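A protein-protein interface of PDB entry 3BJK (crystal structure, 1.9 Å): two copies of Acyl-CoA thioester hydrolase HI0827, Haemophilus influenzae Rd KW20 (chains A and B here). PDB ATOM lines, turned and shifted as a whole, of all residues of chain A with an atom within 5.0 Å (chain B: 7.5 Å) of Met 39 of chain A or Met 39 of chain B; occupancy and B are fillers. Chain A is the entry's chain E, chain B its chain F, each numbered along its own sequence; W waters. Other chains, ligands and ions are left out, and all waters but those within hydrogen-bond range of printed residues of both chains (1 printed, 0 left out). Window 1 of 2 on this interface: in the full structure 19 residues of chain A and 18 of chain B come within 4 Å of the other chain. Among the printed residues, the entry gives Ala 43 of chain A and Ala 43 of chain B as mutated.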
ATOM      1  N   GLY A  35     -13.226  22.108  19.670  1.00  0.00           N
ATOM      2  CA  GLY A  35     -12.597  22.721  18.494  1.00  0.00           C
ATOM      3  C   GLY A  35     -11.186  23.219  18.770  1.00  0.00           C
ATOM      4  O   GLY A  35     -10.326  23.159  17.906  1.00  0.00           O
ATOM      5  N   GLY A  36     -10.933  23.687  19.989  1.00  0.00           N
ATOM      6  CA  GLY A  36      -9.568  24.114  20.391  1.00  0.00           C
ATOM      7  C   GLY A  36      -8.557  22.958  20.312  1.00  0.00           C
ATOM      8  O   GLY A  36      -7.397  23.160  19.945  1.00  0.00           O
ATOM      9  N   TRP A  37      -8.998  21.740  20.620  1.00  0.00           N
ATOM     10  CA  TRP A  37      -8.123  20.569  20.543  1.00  0.00           C
ATOM     11  C   TRP A  37      -7.813  20.220  19.099  1.00  0.00           C
ATOM     12  O   TRP A  37      -6.695  19.822  18.747  1.00  0.00           O
ATOM     13  CB  TRP A  37      -8.761  19.348  21.187  1.00  0.00           C
ATOM     14  CG  TRP A  37      -7.921  18.064  21.133  1.00  0.00           C
ATOM     15  CD1 TRP A  37      -6.986  17.677  22.032  1.00  0.00           C
ATOM     16  CD2 TRP A  37      -8.029  16.994  20.187  1.00  0.00           C
ATOM     17  NE1 TRP A  37      -6.454  16.452  21.678  1.00  0.00           N
ATOM     18  CE2 TRP A  37      -7.084  16.017  20.546  1.00  0.00           C
ATOM     19  CE3 TRP A  37      -8.798  16.792  19.036  1.00  0.00           C
ATOM     20  CZ2 TRP A  37      -6.912  14.838  19.820  1.00  0.00           C
ATOM     21  CZ3 TRP A  37      -8.620  15.618  18.314  1.00  0.00           C
ATOM     22  CH2 TRP A  37      -7.696  14.661  18.722  1.00  0.00           C
ATOM     23  N   ILE A  38      -8.842  20.277  18.277  1.00  0.00           N
ATOM     24  CA  ILE A  38      -8.669  20.072  16.858  1.00  0.00           C
ATOM     25  C   ILE A  38      -7.664  21.092  16.282  1.00  0.00           C
ATOM     26  O   ILE A  38      -6.768  20.715  15.534  1.00  0.00           O
ATOM     27  CB  ILE A  38     -10.018  20.181  16.079  1.00  0.00           C
ATOM     28  CG1 ILE A  38     -11.059  19.231  16.656  1.00  0.00           C
ATOM     29  CG2 ILE A  38      -9.801  19.888  14.603  1.00  0.00           C
ATOM     30  CD1 ILE A  38     -12.334  19.241  15.830  1.00  0.00           C
ATOM     31  N   MET A  39      -7.824  22.374  16.610  1.00  0.00           N
ATOM     32  CA  MET A  39      -6.903  23.405  16.097  1.00  0.00           C
ATOM     33  C   MET A  39      -5.454  23.125  16.555  1.00  0.00           C
ATOM     34  O   MET A  39      -4.465  23.324  15.802  1.00  0.00           O
ATOM     35  CB  MET A  39      -7.331  24.776  16.550  1.00  0.00           C
ATOM     36  CG  MET A  39      -8.683  25.176  16.005  1.00  0.00           C
ATOM     37  SD  MET A  39      -9.245  26.833  16.420  1.00  0.00           S
ATOM     38  CE  MET A  39      -9.507  26.808  18.117  1.00  0.00           C
ATOM     39  N   SER A  40      -5.343  22.677  17.801  1.00  0.00           N
ATOM     40  CA  SER A  40      -4.074  22.235  18.386  1.00  0.00           C
ATOM     41  C   SER A  40      -3.407  21.092  17.640  1.00  0.00           C
ATOM     42  O   SER A  40      -2.179  21.119  17.410  1.00  0.00           O
ATOM     43  CB  SER A  40      -4.284  21.797  19.834  1.00  0.00           C
ATOM     44  OG  SER A  40      -4.533  22.910  20.622  1.00  0.00           O
ATOM     45  N   GLN A  41      -4.199  20.059  17.286  1.00  0.00           N
ATOM     46  CA  GLN A  41      -3.643  18.935  16.513  1.00  0.00           C
ATOM     47  C   GLN A  41      -3.118  19.435  15.172  1.00  0.00           C
ATOM     48  O   GLN A  41      -2.038  19.019  14.700  1.00  0.00           O
ATOM     49  CB  GLN A  41      -4.658  17.793  16.315  1.00  0.00           C
ATOM     50  CG  GLN A  41      -5.157  17.162  17.579  1.00  0.00           C
ATOM     51  CD  GLN A  41      -4.049  16.749  18.549  1.00  0.00           C
ATOM     52  OE1 GLN A  41      -3.305  15.814  18.305  1.00  0.00           O
ATOM     53  NE2 GLN A  41      -3.937  17.484  19.659  1.00  0.00           N
ATOM     54  N   MET A  42      -3.892  20.320  14.544  1.00  0.00           N
ATOM     55  CA  MET A  42      -3.558  20.851  13.210  1.00  0.00           C
ATOM     56  C   MET A  42      -2.232  21.648  13.252  1.00  0.00           C
ATOM     57  O   MET A  42      -1.356  21.493  12.368  1.00  0.00           O
ATOM     58  CB  MET A  42      -4.689  21.735  12.702  1.00  0.00           C
ATOM     59  CG  MET A  42      -5.952  20.976  12.309  1.00  0.00           C
ATOM     60  SD  MET A  42      -7.336  22.031  11.809  1.00  0.00           S
ATOM     61  CE  MET A  42      -6.924  22.213  10.130  1.00  0.00           C
ATOM     62  N   ALA A  43      -2.090  22.469  14.296  1.00  0.00           N
ATOM     63  CA  ALA A  43      -0.889  23.281  14.465  1.00  0.00           C
ATOM     64  C   ALA A  43       0.329  22.403  14.709  1.00  0.00           C
ATOM     65  O   ALA A  43       1.355  22.613  14.079  1.00  0.00           O
ATOM     66  CB  ALA A  43      -1.062  24.283  15.577  1.00  0.00           C
ATOM     67  N   VAL A  63      -3.127  31.533  10.213  1.00  0.00           N
ATOM     68  CA  VAL A  63      -4.125  30.561   9.764  1.00  0.00           C
ATOM     69  C   VAL A  63      -5.109  31.320   8.912  1.00  0.00           C
ATOM     70  O   VAL A  63      -5.516  32.454   9.256  1.00  0.00           O
ATOM     71  CB  VAL A  63      -4.876  29.845  10.946  1.00  0.00           C
ATOM     72  CG1 VAL A  63      -5.851  28.809  10.407  1.00  0.00           C
ATOM     73  CG2 VAL A  63      -3.886  29.220  11.857  1.00  0.00           C
ATOM     74  N   MET A  66      -9.972  28.370   7.819  1.00  0.00           N
ATOM     75  CA  MET A  66     -10.310  27.275   8.686  1.00  0.00           C
ATOM     76  C   MET A  66     -11.813  26.979   8.650  1.00  0.00           C
ATOM     77  O   MET A  66     -12.615  27.875   8.887  1.00  0.00           O
ATOM     78  CB  MET A  66      -9.868  27.558  10.102  1.00  0.00           C
ATOM     79  CG  MET A  66     -10.176  26.416  11.021  1.00  0.00           C
ATOM     80  SD  MET A  66      -9.282  26.524  12.567  1.00  0.00           S
ATOM     81  CE  MET A  66      -7.632  26.017  12.147  1.00  0.00           C
ATOM     82  N   PHE A  68     -14.824  24.218   9.915  1.00  0.00           N
ATOM     83  CA  PHE A  68     -15.226  23.056  10.717  1.00  0.00           C
ATOM     84  C   PHE A  68     -16.367  22.437   9.974  1.00  0.00           C
ATOM     85  O   PHE A  68     -17.399  23.075   9.757  1.00  0.00           O
ATOM     86  CB  PHE A  68     -15.611  23.453  12.154  1.00  0.00           C
ATOM     87  CG  PHE A  68     -14.453  23.996  12.938  1.00  0.00           C
ATOM     88  CD1 PHE A  68     -13.534  23.133  13.512  1.00  0.00           C
ATOM     89  CD2 PHE A  68     -14.252  25.359  13.051  1.00  0.00           C
ATOM     90  CE1 PHE A  68     -12.443  23.621  14.198  1.00  0.00           C
ATOM     91  CE2 PHE A  68     -13.195  25.852  13.766  1.00  0.00           C
ATOM     92  CZ  PHE A  68     -12.292  24.993  14.330  1.00  0.00           C
ATOM     93  N   PHE A 119      -2.231  26.873   7.130  1.00  0.00           N
ATOM     94  CA  PHE A 119      -1.305  27.339   8.160  1.00  0.00           C
ATOM     95  C   PHE A 119      -0.048  27.897   7.523  1.00  0.00           C
ATOM     96  O   PHE A 119       0.462  27.336   6.537  1.00  0.00           O
ATOM     97  CB  PHE A 119      -0.875  26.213   9.073  1.00  0.00           C
ATOM     98  CG  PHE A 119      -1.846  25.890  10.184  1.00  0.00           C
ATOM     99  CD1 PHE A 119      -3.013  25.174   9.923  1.00  0.00           C
ATOM    100  CD2 PHE A 119      -1.591  26.295  11.495  1.00  0.00           C
ATOM    101  CE1 PHE A 119      -3.915  24.851  10.951  1.00  0.00           C
ATOM    102  CE2 PHE A 119      -2.489  25.963  12.537  1.00  0.00           C
ATOM    103  CZ  PHE A 119      -3.654  25.235  12.259  1.00  0.00           C
ATOM    104  N   PHE B  34       2.364  27.493  23.614  1.00  0.00           N
ATOM    105  CA  PHE B  34       1.873  26.772  22.427  1.00  0.00           C
ATOM    106  C   PHE B  34       0.725  27.505  21.716  1.00  0.00           C
ATOM    107  O   PHE B  34      -0.264  27.865  22.352  1.00  0.00           O
ATOM    108  CB  PHE B  34       1.452  25.340  22.898  1.00  0.00           C
ATOM    109  CG  PHE B  34       0.870  24.439  21.810  1.00  0.00           C
ATOM    110  CD1 PHE B  34       1.421  24.384  20.523  1.00  0.00           C
ATOM    111  CD2 PHE B  34      -0.248  23.640  22.085  1.00  0.00           C
ATOM    112  CE1 PHE B  34       0.873  23.531  19.528  1.00  0.00           C
ATOM    113  CE2 PHE B  34      -0.792  22.761  21.096  1.00  0.00           C
ATOM    114  CZ  PHE B  34      -0.242  22.724  19.817  1.00  0.00           C
ATOM    115  N   GLY B  35       0.839  27.671  20.394  1.00  0.00           N
ATOM    116  CA  GLY B  35      -0.191  28.294  19.539  1.00  0.00           C
ATOM    117  C   GLY B  35      -1.573  27.629  19.680  1.00  0.00           C
ATOM    118  O   GLY B  35      -2.575  28.332  19.652  1.00  0.00           O
ATOM    119  N   GLY B  36      -1.565  26.315  19.937  1.00  0.00           N
ATOM    120  CA  GLY B  36      -2.760  25.465  20.149  1.00  0.00           C
ATOM    121  C   GLY B  36      -3.533  25.981  21.326  1.00  0.00           C
ATOM    122  O   GLY B  36      -4.737  26.165  21.254  1.00  0.00           O
ATOM    123  N   TRP B  37      -2.802  26.314  22.392  1.00  0.00           N
ATOM    124  CA  TRP B  37      -3.420  26.857  23.597  1.00  0.00           C
ATOM    125  C   TRP B  37      -4.031  28.235  23.383  1.00  0.00           C
ATOM    126  O   TRP B  37      -5.123  28.522  23.856  1.00  0.00           O
ATOM    127  CB  TRP B  37      -2.351  26.951  24.680  1.00  0.00           C
ATOM    128  CG  TRP B  37      -2.922  27.400  25.987  1.00  0.00           C
ATOM    129  CD1 TRP B  37      -3.515  26.625  26.911  1.00  0.00           C
ATOM    130  CD2 TRP B  37      -2.992  28.746  26.473  1.00  0.00           C
ATOM    131  NE1 TRP B  37      -3.937  27.394  27.989  1.00  0.00           N
ATOM    132  CE2 TRP B  37      -3.587  28.699  27.746  1.00  0.00           C
ATOM    133  CE3 TRP B  37      -2.564  29.984  25.971  1.00  0.00           C
ATOM    134  CZ2 TRP B  37      -3.780  29.839  28.524  1.00  0.00           C
ATOM    135  CZ3 TRP B  37      -2.744  31.103  26.743  1.00  0.00           C
ATOM    136  CH2 TRP B  37      -3.370  31.030  28.010  1.00  0.00           C
ATOM    137  N   ILE B  38      -3.316  29.065  22.638  1.00  0.00           N
ATOM    138  CA  ILE B  38      -3.780  30.421  22.262  1.00  0.00           C
ATOM    139  C   ILE B  38      -5.071  30.346  21.440  1.00  0.00           C
ATOM    140  O   ILE B  38      -6.062  31.003  21.757  1.00  0.00           O
ATOM    141  CB  ILE B  38      -2.687  31.230  21.545  1.00  0.00           C
ATOM    142  CG1 ILE B  38      -1.376  31.256  22.385  1.00  0.00           C
ATOM    143  CG2 ILE B  38      -3.184  32.655  21.281  1.00  0.00           C
ATOM    144  CD1 ILE B  38      -0.159  31.948  21.727  1.00  0.00           C
ATOM    145  N   MET B  39      -5.088  29.471  20.438  1.00  0.00           N
ATOM    146  CA  MET B  39      -6.289  29.252  19.614  1.00  0.00           C
ATOM    147  C   MET B  39      -7.490  28.752  20.438  1.00  0.00           C
ATOM    148  O   MET B  39      -8.649  29.157  20.214  1.00  0.00           O
ATOM    149  CB  MET B  39      -5.964  28.251  18.522  1.00  0.00           C
ATOM    150  CG  MET B  39      -4.943  28.785  17.549  1.00  0.00           C
ATOM    151  SD  MET B  39      -4.722  27.775  16.080  1.00  0.00           S
ATOM    152  CE  MET B  39      -3.687  26.540  16.683  1.00  0.00           C
ATOM    153  N   SER B  40      -7.200  27.841  21.360  1.00  0.00           N
ATOM    154  CA  SER B  40      -8.181  27.331  22.298  1.00  0.00           C
ATOM    155  C   SER B  40      -8.759  28.433  23.173  1.00  0.00           C
ATOM    156  O   SER B  40      -9.951  28.470  23.370  1.00  0.00           O
ATOM    157  CB  SER B  40      -7.594  26.212  23.165  1.00  0.00           C
ATOM    158  OG  SER B  40      -7.412  25.028  22.410  1.00  0.00           O
ATOM    159  N   GLN B  41      -7.921  29.309  23.733  1.00  0.00           N
ATOM    160  CA  GLN B  41      -8.449  30.497  24.476  1.00  0.00           C
ATOM    161  C   GLN B  41      -9.383  31.368  23.626  1.00  0.00           C
ATOM    162  O   GLN B  41     -10.438  31.762  24.090  1.00  0.00           O
ATOM    163  CB  GLN B  41      -7.334  31.373  25.029  1.00  0.00           C
ATOM    164  CG  GLN B  41      -6.564  30.724  26.165  1.00  0.00           C
ATOM    165  CD  GLN B  41      -7.400  30.598  27.454  1.00  0.00           C
ATOM    166  OE1 GLN B  41      -7.744  29.512  27.824  1.00  0.00           O
ATOM    167  NE2 GLN B  41      -7.762  31.733  28.100  1.00  0.00           N
ATOM    168  N   MET B  42      -8.972  31.673  22.396  1.00  0.00           N
ATOM    169  CA  MET B  42      -9.712  32.504  21.489  1.00  0.00           C
ATOM    170  C   MET B  42     -11.091  31.887  21.185  1.00  0.00           C
ATOM    171  O   MET B  42     -12.131  32.584  21.224  1.00  0.00           O
ATOM    172  CB  MET B  42      -8.894  32.727  20.217  1.00  0.00           C
ATOM    173  CG  MET B  42      -7.695  33.670  20.429  1.00  0.00           C
ATOM    174  SD  MET B  42      -6.966  34.321  18.905  1.00  0.00           S
ATOM    175  CE  MET B  42      -6.202  32.841  18.300  1.00  0.00           C
ATOM    176  N   ALA B  43     -11.085  30.580  20.949  1.00  0.00           N
ATOM    177  CA  ALA B  43     -12.309  29.839  20.637  1.00  0.00           C
ATOM    178  C   ALA B  43     -13.252  29.834  21.827  1.00  0.00           C
ATOM    179  O   ALA B  43     -14.450  30.055  21.673  1.00  0.00           O
ATOM    180  CB  ALA B  43     -11.969  28.444  20.229  1.00  0.00           C
ATOM    181  N   MET B  44     -12.714  29.591  23.025  1.00  0.00           N
ATOM    182  CA  MET B  44     -13.533  29.606  24.215  1.00  0.00           C
ATOM    183  C   MET B  44     -14.134  30.984  24.447  1.00  0.00           C
ATOM    184  O   MET B  44     -15.335  31.121  24.734  1.00  0.00           O
ATOM    185  CB  MET B  44     -12.733  29.160  25.413  1.00  0.00           C
ATOM    186  CG  MET B  44     -13.534  29.000  26.704  1.00  0.00           C
ATOM    187  SD  MET B  44     -12.391  28.366  28.012  1.00  0.00           S
ATOM    188  CE  MET B  44     -11.831  26.901  27.178  1.00  0.00           C
ATOM    189  N   GLY B  45     -13.308  32.007  24.312  1.00  0.00           N
ATOM    190  CA  GLY B  45     -13.702  33.355  24.662  1.00  0.00           C
ATOM    191  C   GLY B  45     -14.718  33.875  23.681  1.00  0.00           C
ATOM    192  O   GLY B  45     -15.784  34.341  24.075  1.00  0.00           O
ATOM    193  N   THR B  60     -18.825  26.463  16.415  1.00  0.00           N
ATOM    194  CA  THR B  60     -17.872  27.125  15.552  1.00  0.00           C
ATOM    195  C   THR B  60     -17.889  26.461  14.182  1.00  0.00           C
ATOM    196  O   THR B  60     -17.820  25.233  14.052  1.00  0.00           O
ATOM    197  CB  THR B  60     -16.482  27.065  16.098  1.00  0.00           C
ATOM    198  OG1 THR B  60     -16.534  27.519  17.436  1.00  0.00           O
ATOM    199  CG2 THR B  60     -15.566  27.952  15.273  1.00  0.00           C
ATOM    200  N   VAL B  63     -13.001  29.860  11.033  1.00  0.00           N
ATOM    201  CA  VAL B  63     -12.021  30.847  11.484  1.00  0.00           C
ATOM    202  C   VAL B  63     -11.307  31.309  10.234  1.00  0.00           C
ATOM    203  O   VAL B  63     -10.470  30.640   9.684  1.00  0.00           O
ATOM    204  CB  VAL B  63     -11.021  30.300  12.550  1.00  0.00           C
ATOM    205  CG1 VAL B  63     -10.185  31.450  13.115  1.00  0.00           C
ATOM    206  CG2 VAL B  63     -11.777  29.581  13.648  1.00  0.00           C
ATOM    207  N   MET B  66      -6.413  34.200  11.351  1.00  0.00           N
ATOM    208  CA  MET B  66      -5.722  34.165  12.633  1.00  0.00           C
ATOM    209  C   MET B  66      -4.306  34.677  12.335  1.00  0.00           C
ATOM    210  O   MET B  66      -3.718  34.339  11.311  1.00  0.00           O
ATOM    211  CB  MET B  66      -5.700  32.726  13.146  1.00  0.00           C
ATOM    212  CG  MET B  66      -5.544  32.441  14.582  1.00  0.00           C
ATOM    213  SD  MET B  66      -6.148  30.712  14.694  1.00  0.00           S
ATOM    214  CE  MET B  66      -7.764  30.828  15.398  1.00  0.00           C
ATOM    215  N   PHE B  68      -0.592  35.429  14.479  1.00  0.00           N
ATOM    216  CA  PHE B  68       0.189  35.287  15.684  1.00  0.00           C
ATOM    217  C   PHE B  68       1.265  36.331  15.585  1.00  0.00           C
ATOM    218  O   PHE B  68       2.137  36.255  14.724  1.00  0.00           O
ATOM    219  CB  PHE B  68       0.763  33.889  15.814  1.00  0.00           C
ATOM    220  CG  PHE B  68      -0.288  32.804  15.926  1.00  0.00           C
ATOM    221  CD1 PHE B  68      -0.822  32.229  14.779  1.00  0.00           C
ATOM    222  CD2 PHE B  68      -0.730  32.359  17.159  1.00  0.00           C
ATOM    223  CE1 PHE B  68      -1.791  31.211  14.856  1.00  0.00           C
ATOM    224  CE2 PHE B  68      -1.693  31.363  17.255  1.00  0.00           C
ATOM    225  CZ  PHE B  68      -2.222  30.786  16.089  1.00  0.00           C
ATOM    226  N   CYS B  80      -8.438  37.918  26.396  1.00  0.00           N
ATOM    227  CA  CYS B  80      -9.055  37.839  25.072  1.00  0.00           C
ATOM    228  C   CYS B  80     -10.184  38.860  25.067  1.00  0.00           C
ATOM    229  O   CYS B  80     -10.962  38.917  26.029  1.00  0.00           O
ATOM    230  CB  CYS B  80      -9.624  36.429  24.779  1.00  0.00           C
ATOM    231  SG  CYS B  80      -8.433  35.147  24.648  1.00  0.00           S
ATOM    232  N   VAL B  98      -6.038  38.876  21.384  1.00  0.00           N
ATOM    233  CA  VAL B  98      -5.331  38.408  22.556  1.00  0.00           C
ATOM    234  C   VAL B  98      -4.278  39.430  22.968  1.00  0.00           C
ATOM    235  O   VAL B  98      -3.448  39.850  22.174  1.00  0.00           O
ATOM    236  CB  VAL B  98      -4.674  37.038  22.352  1.00  0.00           C
ATOM    237  CG1 VAL B  98      -4.096  36.526  23.724  1.00  0.00           C
ATOM    238  CG2 VAL B  98      -5.669  36.071  21.786  1.00  0.00           C
ATOM    239  N   THR B 115      -2.037  38.322  19.403  1.00  0.00           N
ATOM    240  CA  THR B 115      -2.754  37.419  18.489  1.00  0.00           C
ATOM    241  C   THR B 115      -4.110  38.033  18.165  1.00  0.00           C
ATOM    242  O   THR B 115      -4.695  38.756  19.002  1.00  0.00           O
ATOM    243  CB  THR B 115      -2.988  36.002  19.119  1.00  0.00           C
ATOM    244  OG1 THR B 115      -1.974  35.686  20.061  1.00  0.00           O
ATOM    245  CG2 THR B 115      -3.074  34.894  18.028  1.00  0.00           C
ATOM    246  N   ALA B 117      -7.898  37.012  15.571  1.00  0.00           N
ATOM    247  CA  ALA B 117      -8.617  36.041  14.753  1.00  0.00           C
ATOM    248  C   ALA B 117     -10.025  36.581  14.524  1.00  0.00           C
ATOM    249  O   ALA B 117     -10.517  37.364  15.338  1.00  0.00           O
ATOM    250  CB  ALA B 117      -8.686  34.690  15.431  1.00  0.00           C
ATOM    251  N   PHE B 119     -13.680  34.770  14.095  1.00  0.00           N
ATOM    252  CA  PHE B 119     -14.473  33.545  14.252  1.00  0.00           C
ATOM    253  C   PHE B 119     -15.911  33.722  13.780  1.00  0.00           C
ATOM    254  O   PHE B 119     -16.548  34.755  13.987  1.00  0.00           O
ATOM    255  CB  PHE B 119     -14.563  33.127  15.721  1.00  0.00           C
ATOM    256  CG  PHE B 119     -13.348  32.441  16.250  1.00  0.00           C
ATOM    257  CD1 PHE B 119     -12.185  33.153  16.512  1.00  0.00           C
ATOM    258  CD2 PHE B 119     -13.381  31.091  16.550  1.00  0.00           C
ATOM    259  CE1 PHE B 119     -11.052  32.498  17.017  1.00  0.00           C
ATOM    260  CE2 PHE B 119     -12.253  30.436  17.042  1.00  0.00           C
ATOM    261  CZ  PHE B 119     -11.093  31.147  17.282  1.00  0.00           C
HETATM  262  O   HOH W   1      -4.106  35.313   8.337  1.00  0.00           O
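Printed residues of chain B that touch a printed residue of chain A: Phe 34, Gly 36, Met 39, Ser 40, Ala 43, Thr 60, Val 63 and Met 66. Hydrophobic or aromatic side chains of chain A that line the printed part of chain B: Met 39, Ala 43, Val 63, Met 66 and Phe 68. Among the printed residues, no Asp or Glu carboxylate lies within 4 Å of a Lys or Arg side-chain nitrogen of the other chain.
Of chain B, only Met 39 (3.3 Å) and Ala 43 (3.6 Å) come within 4 Å of Met 39 of chain A. Of the printed residues of chain B, Met 66 of chain A touches Val 63. Of the printed residues of chain A, Ala 43 of chain B touches Met 39. Of the printed residues of chain A, Met 66 of chain B touches Val 63. The nearest printed residue of chain A that does not touch Met 39 of chain B is Ser 40 of chain A (4.3 Å).
Gly 36 of chain A touches Ser 40 of chain B, and with the chains exchanged Ser 40 of chain A touches Gly 36 of chain B. Met 39 of chain B touches its own counterpart, Met 39 of chain A. Val 63 of chain A touches Met 66 of chain B, and with the chains exchanged Met 66 of chain A touches Val 63 of chain B. Phe 68 of chain A touches Val 63 of chain B, but with the chains exchanged Val 63 of chain A does not touch Phe 68 of chain B (4.2 Å). 13 positions are printed for both chains. Of the 11 pairs that touch across the chains among the printed residues, 8 have their exchanged pair printed and touching as well.
Met 39 of chain B touches Met 39 of chain A. CB of Ala 43 of chain B touches CE of Met 39 of chain A, 3.6 Å away. O of Ser 40 of chain A touches CZ of Phe 34 of chain B, at 3.5 Å. Ser 40 of chain B touches Ser 40 of chain A (OG to OG, 3.996 Å). Met 39 of chain B touches Ala 43 of chain A (CE to CB, 3.6 Å). Thr 60 of chain B touches Phe 68 of chain A. Val 63 of chain B touches Phe 68 of chain A (CG2 to CE2, 3.99 Å).
The backbone carbonyl oxygen of Gly 36 of chain A sits close to the side-chain hydroxyl of Ser 40 of chain B. OG of Ser 40 of chain A lies close to O of Gly 36 of chain B, 3.3 Å away. O of Met 66 of chain A sits at hydrogen-bond distance from N of Val 63 of chain B (2.9 Å). N of Met 66 of chain B lies within hydrogen-bond range of O of Val 63 of chain A.
OG of Ser 40 of chain A is in hydrogen-bond range of O of Gly 36 of chain A. O of Gly 36 of chain B sits at hydrogen-bond distance from OG of Ser 40 of chain B (3.1 Å).
Water W1 lies within hydrogen-bond range of the backbone carbonyl oxygen (O) of Met 66 of chain B (3.2 Å) and the backbone carbonyl oxygen (O) of Val 63 of chain A (3.3 Å).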
